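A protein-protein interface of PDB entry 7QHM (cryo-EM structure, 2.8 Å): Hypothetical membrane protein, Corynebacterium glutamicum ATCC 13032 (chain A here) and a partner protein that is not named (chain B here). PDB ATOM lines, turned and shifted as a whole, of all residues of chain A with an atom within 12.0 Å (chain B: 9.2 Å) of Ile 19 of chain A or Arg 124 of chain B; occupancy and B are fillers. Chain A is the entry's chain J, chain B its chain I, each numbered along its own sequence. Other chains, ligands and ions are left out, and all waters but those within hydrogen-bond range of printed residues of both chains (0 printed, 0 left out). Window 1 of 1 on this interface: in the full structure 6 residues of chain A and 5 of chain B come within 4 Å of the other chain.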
ATOM      1  N   ARG A  15      -0.563  27.962 -33.004  1.00  0.00           N
ATOM      2  CA  ARG A  15      -0.236  27.022 -31.941  1.00  0.00           C
ATOM      3  C   ARG A  15       0.614  25.874 -32.477  1.00  0.00           C
ATOM      4  O   ARG A  15       0.574  25.540 -33.662  1.00  0.00           O
ATOM      5  CB  ARG A  15      -1.518  26.468 -31.315  1.00  0.00           C
ATOM      6  CG  ARG A  15      -2.444  27.519 -30.701  1.00  0.00           C
ATOM      7  CD  ARG A  15      -3.889  27.052 -30.725  1.00  0.00           C
ATOM      8  NE  ARG A  15      -4.801  28.039 -30.158  1.00  0.00           N
ATOM      9  CZ  ARG A  15      -5.239  29.120 -30.789  1.00  0.00           C
ATOM     10  NH1 ARG A  15      -4.832  29.427 -32.012  1.00  0.00           N
ATOM     11  NH2 ARG A  15      -6.108  29.918 -30.178  1.00  0.00           N
ATOM     12  N   MET A  16       1.397  25.274 -31.586  1.00  0.00           N
ATOM     13  CA  MET A  16       2.254  24.165 -31.977  1.00  0.00           C
ATOM     14  C   MET A  16       1.434  22.899 -32.184  1.00  0.00           C
ATOM     15  O   MET A  16       0.370  22.714 -31.587  1.00  0.00           O
ATOM     16  CB  MET A  16       3.325  23.910 -30.917  1.00  0.00           C
ATOM     17  CG  MET A  16       4.223  25.099 -30.641  1.00  0.00           C
ATOM     18  SD  MET A  16       3.343  26.509 -29.947  1.00  0.00           S
ATOM     19  CE  MET A  16       2.904  25.874 -28.332  1.00  0.00           C
ATOM     20  N   HIS A  17       1.953  22.019 -33.035  1.00  0.00           N
ATOM     21  CA  HIS A  17       1.286  20.764 -33.343  1.00  0.00           C
ATOM     22  C   HIS A  17       1.599  19.721 -32.282  1.00  0.00           C
ATOM     23  O   HIS A  17       2.766  19.482 -31.964  1.00  0.00           O
ATOM     24  CB  HIS A  17       1.729  20.261 -34.711  1.00  0.00           C
ATOM     25  CG  HIS A  17       1.299  18.862 -35.003  1.00  0.00           C
ATOM     26  ND1 HIS A  17       0.054  18.384 -34.668  1.00  0.00           N
ATOM     27  CD2 HIS A  17       1.949  17.838 -35.597  1.00  0.00           C
ATOM     28  CE1 HIS A  17      -0.047  17.123 -35.044  1.00  0.00           C
ATOM     29  NE2 HIS A  17       1.090  16.768 -35.612  1.00  0.00           N
ATOM     30  N   TYR A  18       0.555  19.100 -31.740  1.00  0.00           N
ATOM     31  CA  TYR A  18       0.683  18.027 -30.765  1.00  0.00           C
ATOM     32  C   TYR A  18      -0.231  16.890 -31.175  1.00  0.00           C
ATOM     33  O   TYR A  18      -1.426  17.103 -31.399  1.00  0.00           O
ATOM     34  CB  TYR A  18       0.307  18.489 -29.353  1.00  0.00           C
ATOM     35  CG  TYR A  18       1.124  19.634 -28.793  1.00  0.00           C
ATOM     36  CD1 TYR A  18       2.489  19.701 -28.981  1.00  0.00           C
ATOM     37  CD2 TYR A  18       0.517  20.639 -28.064  1.00  0.00           C
ATOM     38  CE1 TYR A  18       3.229  20.737 -28.468  1.00  0.00           C
ATOM     39  CE2 TYR A  18       1.246  21.678 -27.550  1.00  0.00           C
ATOM     40  CZ  TYR A  18       2.603  21.724 -27.758  1.00  0.00           C
ATOM     41  OH  TYR A  18       3.337  22.764 -27.238  1.00  0.00           O
ATOM     42  N   ILE A  19       0.326  15.687 -31.268  1.00  0.00           N
ATOM     43  CA  ILE A  19      -0.481  14.515 -31.569  1.00  0.00           C
ATOM     44  C   ILE A  19      -1.274  14.105 -30.334  1.00  0.00           C
ATOM     45  O   ILE A  19      -0.983  14.513 -29.208  1.00  0.00           O
ATOM     46  CB  ILE A  19       0.390  13.358 -32.089  1.00  0.00           C
ATOM     47  CG1 ILE A  19       1.388  12.878 -31.022  1.00  0.00           C
ATOM     48  CG2 ILE A  19       1.103  13.794 -33.359  1.00  0.00           C
ATOM     49  CD1 ILE A  19       2.238  11.711 -31.444  1.00  0.00           C
ATOM     50  N   LYS A  20      -2.294  13.284 -30.550  1.00  0.00           N
ATOM     51  CA  LYS A  20      -3.040  12.734 -29.433  1.00  0.00           C
ATOM     52  C   LYS A  20      -2.128  11.836 -28.617  1.00  0.00           C
ATOM     53  O   LYS A  20      -1.422  10.986 -29.168  1.00  0.00           O
ATOM     54  CB  LYS A  20      -4.253  11.956 -29.936  1.00  0.00           C
ATOM     55  CG  LYS A  20      -5.054  11.271 -28.841  1.00  0.00           C
ATOM     56  CD  LYS A  20      -6.396  10.790 -29.356  1.00  0.00           C
ATOM     57  CE  LYS A  20      -7.189  10.096 -28.262  1.00  0.00           C
ATOM     58  NZ  LYS A  20      -8.511   9.615 -28.751  1.00  0.00           N
ATOM     59  N   GLY A  21      -2.126  12.038 -27.305  1.00  0.00           N
ATOM     60  CA  GLY A  21      -1.283  11.271 -26.414  1.00  0.00           C
ATOM     61  C   GLY A  21       0.083  11.859 -26.149  1.00  0.00           C
ATOM     62  O   GLY A  21       0.943  11.147 -25.616  1.00  0.00           O
ATOM     63  N   TYR A  22       0.313  13.123 -26.505  1.00  0.00           N
ATOM     64  CA  TYR A  22       1.572  13.812 -26.255  1.00  0.00           C
ATOM     65  C   TYR A  22       1.351  14.937 -25.257  1.00  0.00           C
ATOM     66  O   TYR A  22       0.334  15.633 -25.305  1.00  0.00           O
ATOM     67  CB  TYR A  22       2.158  14.371 -27.547  1.00  0.00           C
ATOM     68  CG  TYR A  22       3.407  15.196 -27.352  1.00  0.00           C
ATOM     69  CD1 TYR A  22       4.591  14.618 -26.924  1.00  0.00           C
ATOM     70  CD2 TYR A  22       3.406  16.554 -27.615  1.00  0.00           C
ATOM     71  CE1 TYR A  22       5.731  15.372 -26.755  1.00  0.00           C
ATOM     72  CE2 TYR A  22       4.542  17.313 -27.450  1.00  0.00           C
ATOM     73  CZ  TYR A  22       5.697  16.719 -27.022  1.00  0.00           C
ATOM     74  OH  TYR A  22       6.822  17.486 -26.862  1.00  0.00           O
ATOM     75  N   VAL A  23       2.316  15.109 -24.364  1.00  0.00           N
ATOM     76  CA  VAL A  23       2.227  16.059 -23.259  1.00  0.00           C
ATOM     77  C   VAL A  23       3.523  16.865 -23.245  1.00  0.00           C
ATOM     78  O   VAL A  23       4.588  16.287 -22.991  1.00  0.00           O
ATOM     79  CB  VAL A  23       1.997  15.331 -21.926  1.00  0.00           C
ATOM     80  CG1 VAL A  23       1.890  16.327 -20.778  1.00  0.00           C
ATOM     81  CG2 VAL A  23       0.748  14.472 -21.998  1.00  0.00           C
ATOM     82  N   PRO A  24       3.502  18.179 -23.520  1.00  0.00           N
ATOM     83  CA  PRO A  24       4.753  18.941 -23.510  1.00  0.00           C
ATOM     84  C   PRO A  24       5.039  19.589 -22.167  1.00  0.00           C
ATOM     85  O   PRO A  24       4.231  19.505 -21.238  1.00  0.00           O
ATOM     86  CB  PRO A  24       4.494  19.999 -24.579  1.00  0.00           C
ATOM     87  CG  PRO A  24       3.071  20.319 -24.358  1.00  0.00           C
ATOM     88  CD  PRO A  24       2.399  19.019 -24.015  1.00  0.00           C
ATOM     89  N   VAL A  25       6.197  20.229 -22.053  1.00  0.00           N
ATOM     90  CA  VAL A  25       6.463  21.207 -21.008  1.00  0.00           C
ATOM     91  C   VAL A  25       6.912  22.477 -21.712  1.00  0.00           C
ATOM     92  O   VAL A  25       7.898  22.462 -22.456  1.00  0.00           O
ATOM     93  CB  VAL A  25       7.515  20.729 -19.985  1.00  0.00           C
ATOM     94  CG1 VAL A  25       6.894  19.733 -19.014  1.00  0.00           C
ATOM     95  CG2 VAL A  25       8.744  20.114 -20.659  1.00  0.00           C
ATOM     96  N   TYR A 104      -6.952  29.652 -23.689  1.00  0.00           N
ATOM     97  CA  TYR A 104      -6.345  28.503 -24.347  1.00  0.00           C
ATOM     98  C   TYR A 104      -6.825  27.201 -23.720  1.00  0.00           C
ATOM     99  O   TYR A 104      -7.218  26.265 -24.423  1.00  0.00           O
ATOM    100  CB  TYR A 104      -4.824  28.610 -24.272  1.00  0.00           C
ATOM    101  CG  TYR A 104      -4.088  27.425 -24.851  1.00  0.00           C
ATOM    102  CD1 TYR A 104      -3.814  27.348 -26.209  1.00  0.00           C
ATOM    103  CD2 TYR A 104      -3.651  26.390 -24.038  1.00  0.00           C
ATOM    104  CE1 TYR A 104      -3.133  26.270 -26.739  1.00  0.00           C
ATOM    105  CE2 TYR A 104      -2.974  25.307 -24.562  1.00  0.00           C
ATOM    106  CZ  TYR A 104      -2.716  25.255 -25.912  1.00  0.00           C
ATOM    107  OH  TYR A 104      -2.042  24.182 -26.436  1.00  0.00           O
ATOM    108  N   THR A 108      -8.673  24.232 -25.646  1.00  0.00           N
ATOM    109  CA  THR A 108      -7.915  23.031 -25.966  1.00  0.00           C
ATOM    110  C   THR A 108      -7.768  22.153 -24.725  1.00  0.00           C
ATOM    111  O   THR A 108      -8.049  22.566 -23.597  1.00  0.00           O
ATOM    112  CB  THR A 108      -6.540  23.391 -26.537  1.00  0.00           C
ATOM    113  OG1 THR A 108      -5.774  24.089 -25.552  1.00  0.00           O
ATOM    114  CG2 THR A 108      -6.691  24.277 -27.748  1.00  0.00           C
ATOM    115  N   GLY A 109      -7.309  20.923 -24.951  1.00  0.00           N
ATOM    116  CA  GLY A 109      -7.373  19.913 -23.912  1.00  0.00           C
ATOM    117  C   GLY A 109      -6.245  19.973 -22.907  1.00  0.00           C
ATOM    118  O   GLY A 109      -6.435  19.606 -21.743  1.00  0.00           O
ATOM    119  N   ARG A 110      -5.069  20.420 -23.326  1.00  0.00           N
ATOM    120  CA  ARG A 110      -3.923  20.428 -22.433  1.00  0.00           C
ATOM    121  C   ARG A 110      -4.087  21.477 -21.342  1.00  0.00           C
ATOM    122  O   ARG A 110      -4.724  22.516 -21.537  1.00  0.00           O
ATOM    123  CB  ARG A 110      -2.635  20.707 -23.207  1.00  0.00           C
ATOM    124  CG  ARG A 110      -2.016  19.494 -23.869  1.00  0.00           C
ATOM    125  CD  ARG A 110      -2.721  19.124 -25.156  1.00  0.00           C
ATOM    126  NE  ARG A 110      -2.141  17.922 -25.738  1.00  0.00           N
ATOM    127  CZ  ARG A 110      -2.426  17.449 -26.943  1.00  0.00           C
ATOM    128  NH1 ARG A 110      -3.272  18.065 -27.750  1.00  0.00           N
ATOM    129  NH2 ARG A 110      -1.849  16.322 -27.348  1.00  0.00           N
ATOM    130  N   THR A 111      -3.513  21.182 -20.176  1.00  0.00           N
ATOM    131  CA  THR A 111      -3.211  22.209 -19.190  1.00  0.00           C
ATOM    132  C   THR A 111      -1.807  22.755 -19.372  1.00  0.00           C
ATOM    133  O   THR A 111      -1.554  23.922 -19.055  1.00  0.00           O
ATOM    134  CB  THR A 111      -3.343  21.662 -17.770  1.00  0.00           C
ATOM    135  OG1 THR A 111      -2.373  20.630 -17.565  1.00  0.00           O
ATOM    136  CG2 THR A 111      -4.742  21.111 -17.521  1.00  0.00           C
ATOM    137  N   GLN A 112      -0.894  21.937 -19.881  1.00  0.00           N
ATOM    138  CA  GLN A 112       0.469  22.372 -20.128  1.00  0.00           C
ATOM    139  C   GLN A 112       0.467  23.395 -21.254  1.00  0.00           C
ATOM    140  O   GLN A 112      -0.392  23.358 -22.134  1.00  0.00           O
ATOM    141  CB  GLN A 112       1.368  21.183 -20.485  1.00  0.00           C
ATOM    142  CG  GLN A 112       1.255  19.993 -19.533  1.00  0.00           C
ATOM    143  CD  GLN A 112       1.411  20.382 -18.075  1.00  0.00           C
ATOM    144  OE1 GLN A 112       2.210  21.252 -17.734  1.00  0.00           O
ATOM    145  NE2 GLN A 112       0.640  19.737 -17.205  1.00  0.00           N
ATOM    146  OXT GLN A 112       1.317  24.283 -21.308  1.00  0.00           O
ATOM    147  N   LEU B 111      15.856   7.343 -34.632  1.00  0.00           N
ATOM    148  CA  LEU B 111      15.109   6.308 -33.913  1.00  0.00           C
ATOM    149  C   LEU B 111      15.698   4.920 -34.159  1.00  0.00           C
ATOM    150  O   LEU B 111      15.028   3.999 -34.628  1.00  0.00           O
ATOM    151  CB  LEU B 111      13.624   6.333 -34.281  1.00  0.00           C
ATOM    152  CG  LEU B 111      12.712   7.416 -33.714  1.00  0.00           C
ATOM    153  CD1 LEU B 111      11.308   7.202 -34.256  1.00  0.00           C
ATOM    154  CD2 LEU B 111      12.692   7.401 -32.190  1.00  0.00           C
ATOM    155  N   TRP B 115      17.567   4.412 -29.100  1.00  0.00           N
ATOM    156  CA  TRP B 115      16.208   4.863 -29.361  1.00  0.00           C
ATOM    157  C   TRP B 115      15.452   3.914 -30.285  1.00  0.00           C
ATOM    158  O   TRP B 115      14.471   4.316 -30.918  1.00  0.00           O
ATOM    159  CB  TRP B 115      16.246   6.267 -29.958  1.00  0.00           C
ATOM    160  CG  TRP B 115      16.434   7.329 -28.960  1.00  0.00           C
ATOM    161  CD1 TRP B 115      17.593   7.678 -28.341  1.00  0.00           C
ATOM    162  CD2 TRP B 115      15.432   8.211 -28.467  1.00  0.00           C
ATOM    163  NE1 TRP B 115      17.372   8.725 -27.487  1.00  0.00           N
ATOM    164  CE2 TRP B 115      16.049   9.073 -27.550  1.00  0.00           C
ATOM    165  CE3 TRP B 115      14.071   8.357 -28.719  1.00  0.00           C
ATOM    166  CZ2 TRP B 115      15.353  10.063 -26.879  1.00  0.00           C
ATOM    167  CZ3 TRP B 115      13.384   9.333 -28.057  1.00  0.00           C
ATOM    168  CH2 TRP B 115      14.023  10.179 -27.145  1.00  0.00           C
ATOM    169  N   LEU B 118      11.423   1.686 -28.678  1.00  0.00           N
ATOM    170  CA  LEU B 118      10.396   2.441 -27.981  1.00  0.00           C
ATOM    171  C   LEU B 118       9.030   1.825 -28.234  1.00  0.00           C
ATOM    172  O   LEU B 118       8.769   1.254 -29.294  1.00  0.00           O
ATOM    173  CB  LEU B 118      10.390   3.903 -28.425  1.00  0.00           C
ATOM    174  CG  LEU B 118      11.405   4.829 -27.755  1.00  0.00           C
ATOM    175  CD1 LEU B 118      12.774   4.643 -28.361  1.00  0.00           C
ATOM    176  CD2 LEU B 118      10.959   6.271 -27.867  1.00  0.00           C
ATOM    177  N   THR B 119       8.155   1.942 -27.243  1.00  0.00           N
ATOM    178  CA  THR B 119       6.828   1.371 -27.353  1.00  0.00           C
ATOM    179  C   THR B 119       5.930   2.294 -28.174  1.00  0.00           C
ATOM    180  O   THR B 119       6.332   3.372 -28.613  1.00  0.00           O
ATOM    181  CB  THR B 119       6.240   1.118 -25.968  1.00  0.00           C
ATOM    182  OG1 THR B 119       6.151   2.350 -25.248  1.00  0.00           O
ATOM    183  CG2 THR B 119       7.107   0.142 -25.190  1.00  0.00           C
ATOM    184  N   ASP B 120       4.694   1.852 -28.395  1.00  0.00           N
ATOM    185  CA  ASP B 120       3.712   2.697 -29.061  1.00  0.00           C
ATOM    186  C   ASP B 120       3.427   3.943 -28.235  1.00  0.00           C
ATOM    187  O   ASP B 120       3.415   5.061 -28.758  1.00  0.00           O
ATOM    188  CB  ASP B 120       2.430   1.895 -29.302  1.00  0.00           C
ATOM    189  CG  ASP B 120       1.372   2.679 -30.060  1.00  0.00           C
ATOM    190  OD1 ASP B 120       0.823   3.658 -29.507  1.00  0.00           O
ATOM    191  OD2 ASP B 120       1.091   2.313 -31.220  1.00  0.00           O
ATOM    192  N   SER B 121       3.186   3.762 -26.937  1.00  0.00           N
ATOM    193  CA  SER B 121       2.906   4.894 -26.063  1.00  0.00           C
ATOM    194  C   SER B 121       4.109   5.815 -25.933  1.00  0.00           C
ATOM    195  O   SER B 121       3.938   7.023 -25.748  1.00  0.00           O
ATOM    196  CB  SER B 121       2.481   4.394 -24.687  1.00  0.00           C
ATOM    197  OG  SER B 121       1.345   3.550 -24.778  1.00  0.00           O
ATOM    198  N   GLN B 122       5.323   5.271 -26.022  1.00  0.00           N
ATOM    199  CA  GLN B 122       6.515   6.098 -25.885  1.00  0.00           C
ATOM    200  C   GLN B 122       6.755   6.927 -27.138  1.00  0.00           C
ATOM    201  O   GLN B 122       7.055   8.123 -27.050  1.00  0.00           O
ATOM    202  CB  GLN B 122       7.726   5.222 -25.568  1.00  0.00           C
ATOM    203  CG  GLN B 122       7.716   4.696 -24.143  1.00  0.00           C
ATOM    204  CD  GLN B 122       8.730   3.598 -23.900  1.00  0.00           C
ATOM    205  OE1 GLN B 122       9.729   3.487 -24.608  1.00  0.00           O
ATOM    206  NE2 GLN B 122       8.483   2.786 -22.880  1.00  0.00           N
ATOM    207  N   LEU B 123       6.643   6.309 -28.315  1.00  0.00           N
ATOM    208  CA  LEU B 123       6.722   7.071 -29.557  1.00  0.00           C
ATOM    209  C   LEU B 123       5.662   8.160 -29.584  1.00  0.00           C
ATOM    210  O   LEU B 123       5.917   9.285 -30.029  1.00  0.00           O
ATOM    211  CB  LEU B 123       6.551   6.141 -30.753  1.00  0.00           C
ATOM    212  CG  LEU B 123       7.642   5.093 -30.931  1.00  0.00           C
ATOM    213  CD1 LEU B 123       7.142   3.974 -31.822  1.00  0.00           C
ATOM    214  CD2 LEU B 123       8.909   5.715 -31.504  1.00  0.00           C
ATOM    215  N   ARG B 124       4.467   7.839 -29.098  1.00  0.00           N
ATOM    216  CA  ARG B 124       3.407   8.828 -29.012  1.00  0.00           C
ATOM    217  C   ARG B 124       3.753   9.925 -28.016  1.00  0.00           C
ATOM    218  O   ARG B 124       3.282  11.057 -28.157  1.00  0.00           O
ATOM    219  CB  ARG B 124       2.111   8.131 -28.624  1.00  0.00           C
ATOM    220  CG  ARG B 124       0.856   8.838 -29.040  1.00  0.00           C
ATOM    221  CD  ARG B 124      -0.366   8.036 -28.636  1.00  0.00           C
ATOM    222  NE  ARG B 124      -0.427   6.756 -29.333  1.00  0.00           N
ATOM    223  CZ  ARG B 124      -0.818   6.593 -30.590  1.00  0.00           C
ATOM    224  NH1 ARG B 124      -1.213   7.615 -31.335  1.00  0.00           N
ATOM    225  NH2 ARG B 124      -0.804   5.375 -31.119  1.00  0.00           N
ATOM    226  N   SER B 125       4.569   9.613 -27.006  1.00  0.00           N
ATOM    227  CA  SER B 125       4.961  10.601 -26.008  1.00  0.00           C
ATOM    228  C   SER B 125       6.149  11.455 -26.432  1.00  0.00           C
ATOM    229  O   SER B 125       6.522  12.353 -25.676  1.00  0.00           O
ATOM    230  CB  SER B 125       5.290   9.915 -24.685  1.00  0.00           C
ATOM    231  OG  SER B 125       5.391  10.871 -23.645  1.00  0.00           O
ATOM    232  N   VAL B 126       6.763  11.189 -27.584  1.00  0.00           N
ATOM    233  CA  VAL B 126       7.768  12.085 -28.156  1.00  0.00           C
ATOM    234  C   VAL B 126       7.216  12.702 -29.433  1.00  0.00           C
ATOM    235  O   VAL B 126       7.974  13.024 -30.354  1.00  0.00           O
ATOM    236  CB  VAL B 126       9.103  11.370 -28.431  1.00  0.00           C
ATOM    237  CG1 VAL B 126       9.714  10.882 -27.133  1.00  0.00           C
ATOM    238  CG2 VAL B 126       8.940  10.223 -29.409  1.00  0.00           C
ATOM    239  N   ASN B 127       5.894  12.859 -29.497  1.00  0.00           N
ATOM    240  CA  ASN B 127       5.219  13.567 -30.583  1.00  0.00           C
ATOM    241  C   ASN B 127       5.479  12.934 -31.947  1.00  0.00           C
ATOM    242  O   ASN B 127       5.507  13.628 -32.961  1.00  0.00           O
ATOM    243  CB  ASN B 127       5.617  15.045 -30.593  1.00  0.00           C
ATOM    244  CG  ASN B 127       4.527  15.944 -31.144  1.00  0.00           C
ATOM    245  OD1 ASN B 127       3.440  15.495 -31.485  1.00  0.00           O
ATOM    246  ND2 ASN B 127       4.814  17.233 -31.221  1.00  0.00           N
ATOM    247  N   ILE B 128       5.650  11.615 -31.987  1.00  0.00           N
ATOM    248  CA  ILE B 128       5.716  10.848 -33.228  1.00  0.00           C
ATOM    249  C   ILE B 128       4.542   9.885 -33.224  1.00  0.00           C
ATOM    250  O   ILE B 128       4.448   9.024 -32.340  1.00  0.00           O
ATOM    251  CB  ILE B 128       7.040  10.080 -33.373  1.00  0.00           C
ATOM    252  CG1 ILE B 128       8.213  11.054 -33.438  1.00  0.00           C
ATOM    253  CG2 ILE B 128       7.013   9.195 -34.625  1.00  0.00           C
ATOM    254  CD1 ILE B 128       9.550  10.422 -33.247  1.00  0.00           C
ATOM    255  N   GLU B 129       3.661  10.017 -34.201  1.00  0.00           N
ATOM    256  CA  GLU B 129       2.575   9.059 -34.347  1.00  0.00           C
ATOM    257  C   GLU B 129       3.159   7.743 -34.854  1.00  0.00           C
ATOM    258  O   GLU B 129       3.769   7.740 -35.929  1.00  0.00           O
ATOM    259  CB  GLU B 129       1.520   9.583 -35.312  1.00  0.00           C
ATOM    260  CG  GLU B 129       0.093   9.228 -34.912  1.00  0.00           C
ATOM    261  CD  GLU B 129      -0.165   7.734 -34.917  1.00  0.00           C
ATOM    262  OE1 GLU B 129       0.371   7.038 -35.803  1.00  0.00           O
ATOM    263  OE2 GLU B 129      -0.902   7.256 -34.031  1.00  0.00           O
ATOM    264  N   PRO B 130       3.008   6.614 -34.141  1.00  0.00           N
ATOM    265  CA  PRO B 130       3.731   5.391 -34.539  1.00  0.00           C
ATOM    266  C   PRO B 130       3.428   4.866 -35.933  1.00  0.00           C
ATOM    267  O   PRO B 130       4.160   3.987 -36.399  1.00  0.00           O
ATOM    268  CB  PRO B 130       3.301   4.367 -33.483  1.00  0.00           C
ATOM    269  CG  PRO B 130       2.942   5.161 -32.316  1.00  0.00           C
ATOM    270  CD  PRO B 130       2.329   6.416 -32.845  1.00  0.00           C
ATOM    271  N   SER B 131       2.379   5.335 -36.606  1.00  0.00           N
ATOM    272  CA  SER B 131       2.202   4.966 -38.005  1.00  0.00           C
ATOM    273  C   SER B 131       3.266   5.594 -38.893  1.00  0.00           C
ATOM    274  O   SER B 131       3.529   5.081 -39.983  1.00  0.00           O
ATOM    275  CB  SER B 131       0.812   5.380 -38.492  1.00  0.00           C
ATOM    276  OG  SER B 131       0.649   6.786 -38.460  1.00  0.00           O
ATOM    277  N   ARG B 132       3.881   6.686 -38.448  1.00  0.00           N
ATOM    278  CA  ARG B 132       4.902   7.361 -39.233  1.00  0.00           C
ATOM    279  C   ARG B 132       6.186   6.555 -39.329  1.00  0.00           C
ATOM    280  O   ARG B 132       6.959   6.762 -40.271  1.00  0.00           O
ATOM    281  CB  ARG B 132       5.192   8.725 -38.605  1.00  0.00           C
ATOM    282  CG  ARG B 132       5.937   9.705 -39.480  1.00  0.00           C
ATOM    283  CD  ARG B 132       6.379  10.894 -38.654  1.00  0.00           C
ATOM    284  NE  ARG B 132       6.472  12.117 -39.445  1.00  0.00           N
ATOM    285  CZ  ARG B 132       7.511  12.467 -40.195  1.00  0.00           C
ATOM    286  NH1 ARG B 132       8.579  11.693 -40.315  1.00  0.00           N
ATOM    287  NH2 ARG B 132       7.477  13.628 -40.842  1.00  0.00           N
ATOM    288  N   VAL B 133       6.420   5.644 -38.388  1.00  0.00           N
ATOM    289  CA  VAL B 133       7.690   4.935 -38.268  1.00  0.00           C
ATOM    290  C   VAL B 133       7.533   3.425 -38.372  1.00  0.00           C
ATOM    291  O   VAL B 133       8.550   2.718 -38.448  1.00  0.00           O
ATOM    292  CB  VAL B 133       8.402   5.314 -36.948  1.00  0.00           C
ATOM    293  CG1 VAL B 133       7.573   4.894 -35.727  1.00  0.00           C
ATOM    294  CG2 VAL B 133       9.829   4.754 -36.877  1.00  0.00           C
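Of the printed residues of chain B, Ile 19 of chain A touches Arg 124, Asn 127, Ile 128 and Glu 129. Arg 124 of chain B touches four residues of chain A. Gly 21 of chain A touches just one residue of chain B: Arg 124 (3.5 Å). No residue of chain A comes within 4 Å of Asp 120 of chain B. No residue of chain A comes within 4 Å of Ser 121 of chain B. Ser 125 of chain B touches just one residue of chain A: Tyr 22. No residue of chain A comes within 4 Å of Val 126 of chain B. Asn 127 of chain B touches just these residues of chain A: His 17 (3.1 Å), Tyr 18 (3.8 Å), Ile 19 (3.1 Å) and Tyr 22 (3.4 Å). Ile 128 of chain B touches just one residue of chain A: Ile 19. Of chain A, only Ile 19 comes within 4 Å of Glu 129 of chain B. No residue of chain A comes within 4 Å of Pro 130 of chain B. Of the printed residues of chain B, Lys 20 of chain A touches Arg 124. Printed residues of chain B within 4 Å of Tyr 22 of chain A: Arg 124 (3.6 Å), Ser 125 (3.2 Å) and Asn 127 (3.4 Å). Of the printed residues of chain B, His 17 of chain A touches Asn 127. Tyr 104 of chain A touches none of the printed residues of chain B. The nearest residue of chain B that does not touch Ile 19 of chain A is Leu 123 of chain B (4.6 Å).
Among the printed residues, merely in contact across the chains: Tyr 18 of chain A with Asn 127 of chain B, Ile 19 of chain A with Arg 124 of chain B, Ile 19 of chain A with Ile 128 of chain B, Ile 19 of chain A with Glu 129 of chain B, Lys 20 of chain A with Arg 124 of chain B, Tyr 22 of chain A with Arg 124 of chain B, Tyr 22 of chain A with Ser 125 of chain B and Tyr 22 of chain A with Asn 127 of chain B.
The side-chain amide oxygen (OD1) of Asn 127 of chain B is in hydrogen-bond range of the backbone NH (N) of Ile 19 of chain A. ND2 of Asn 127 of chain B sits at hydrogen-bond distance from O of His 17 of chain A (3.1 Å). The backbone carbonyl oxygen (O) of Gly 21 of chain A lies close to the backbone carbonyl oxygen (O) of Arg 124 of chain B (3.5 Å).
The guanidinium group of Arg 110 of chain A lies within hydrogen-bond range of the backbone carbonyl oxygen of Ile 19 of chain A. OD1 of Asp 120 of chain B lies within salt-bridge range of NH2 of Arg 124 of chain B (2.9 Å). The backbone carbonyl oxygen (O) of Leu 123 of chain B sits at hydrogen-bond distance from the backbone NH (N) of Ile 128 of chain B (3.1 Å). The side-chain carboxylate (OE1) of Glu 129 of chain B sits at hydrogen-bond distance from the side-chain hydroxyl (OG) of Ser 131 of chain B (2.7 Å). The guanidinium group (NH1) of Arg 124 of chain B is in salt-bridge range of the side-chain carboxylate (OE2) of Glu 129 of chain B. The backbone carbonyl oxygen (O) of Tyr 22 of chain A lies within hydrogen-bond range of the guanidinium group (NH2) of Arg 110 of chain A.
Printed residues of chain B that touch a printed residue of chain A: Arg 124, Ser 125, Asn 127, Ile 128 and Glu 129. Among the printed residues, no Asp or Glu carboxylate lies within 4 Å of a Lys or Arg side-chain nitrogen of the other chain.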
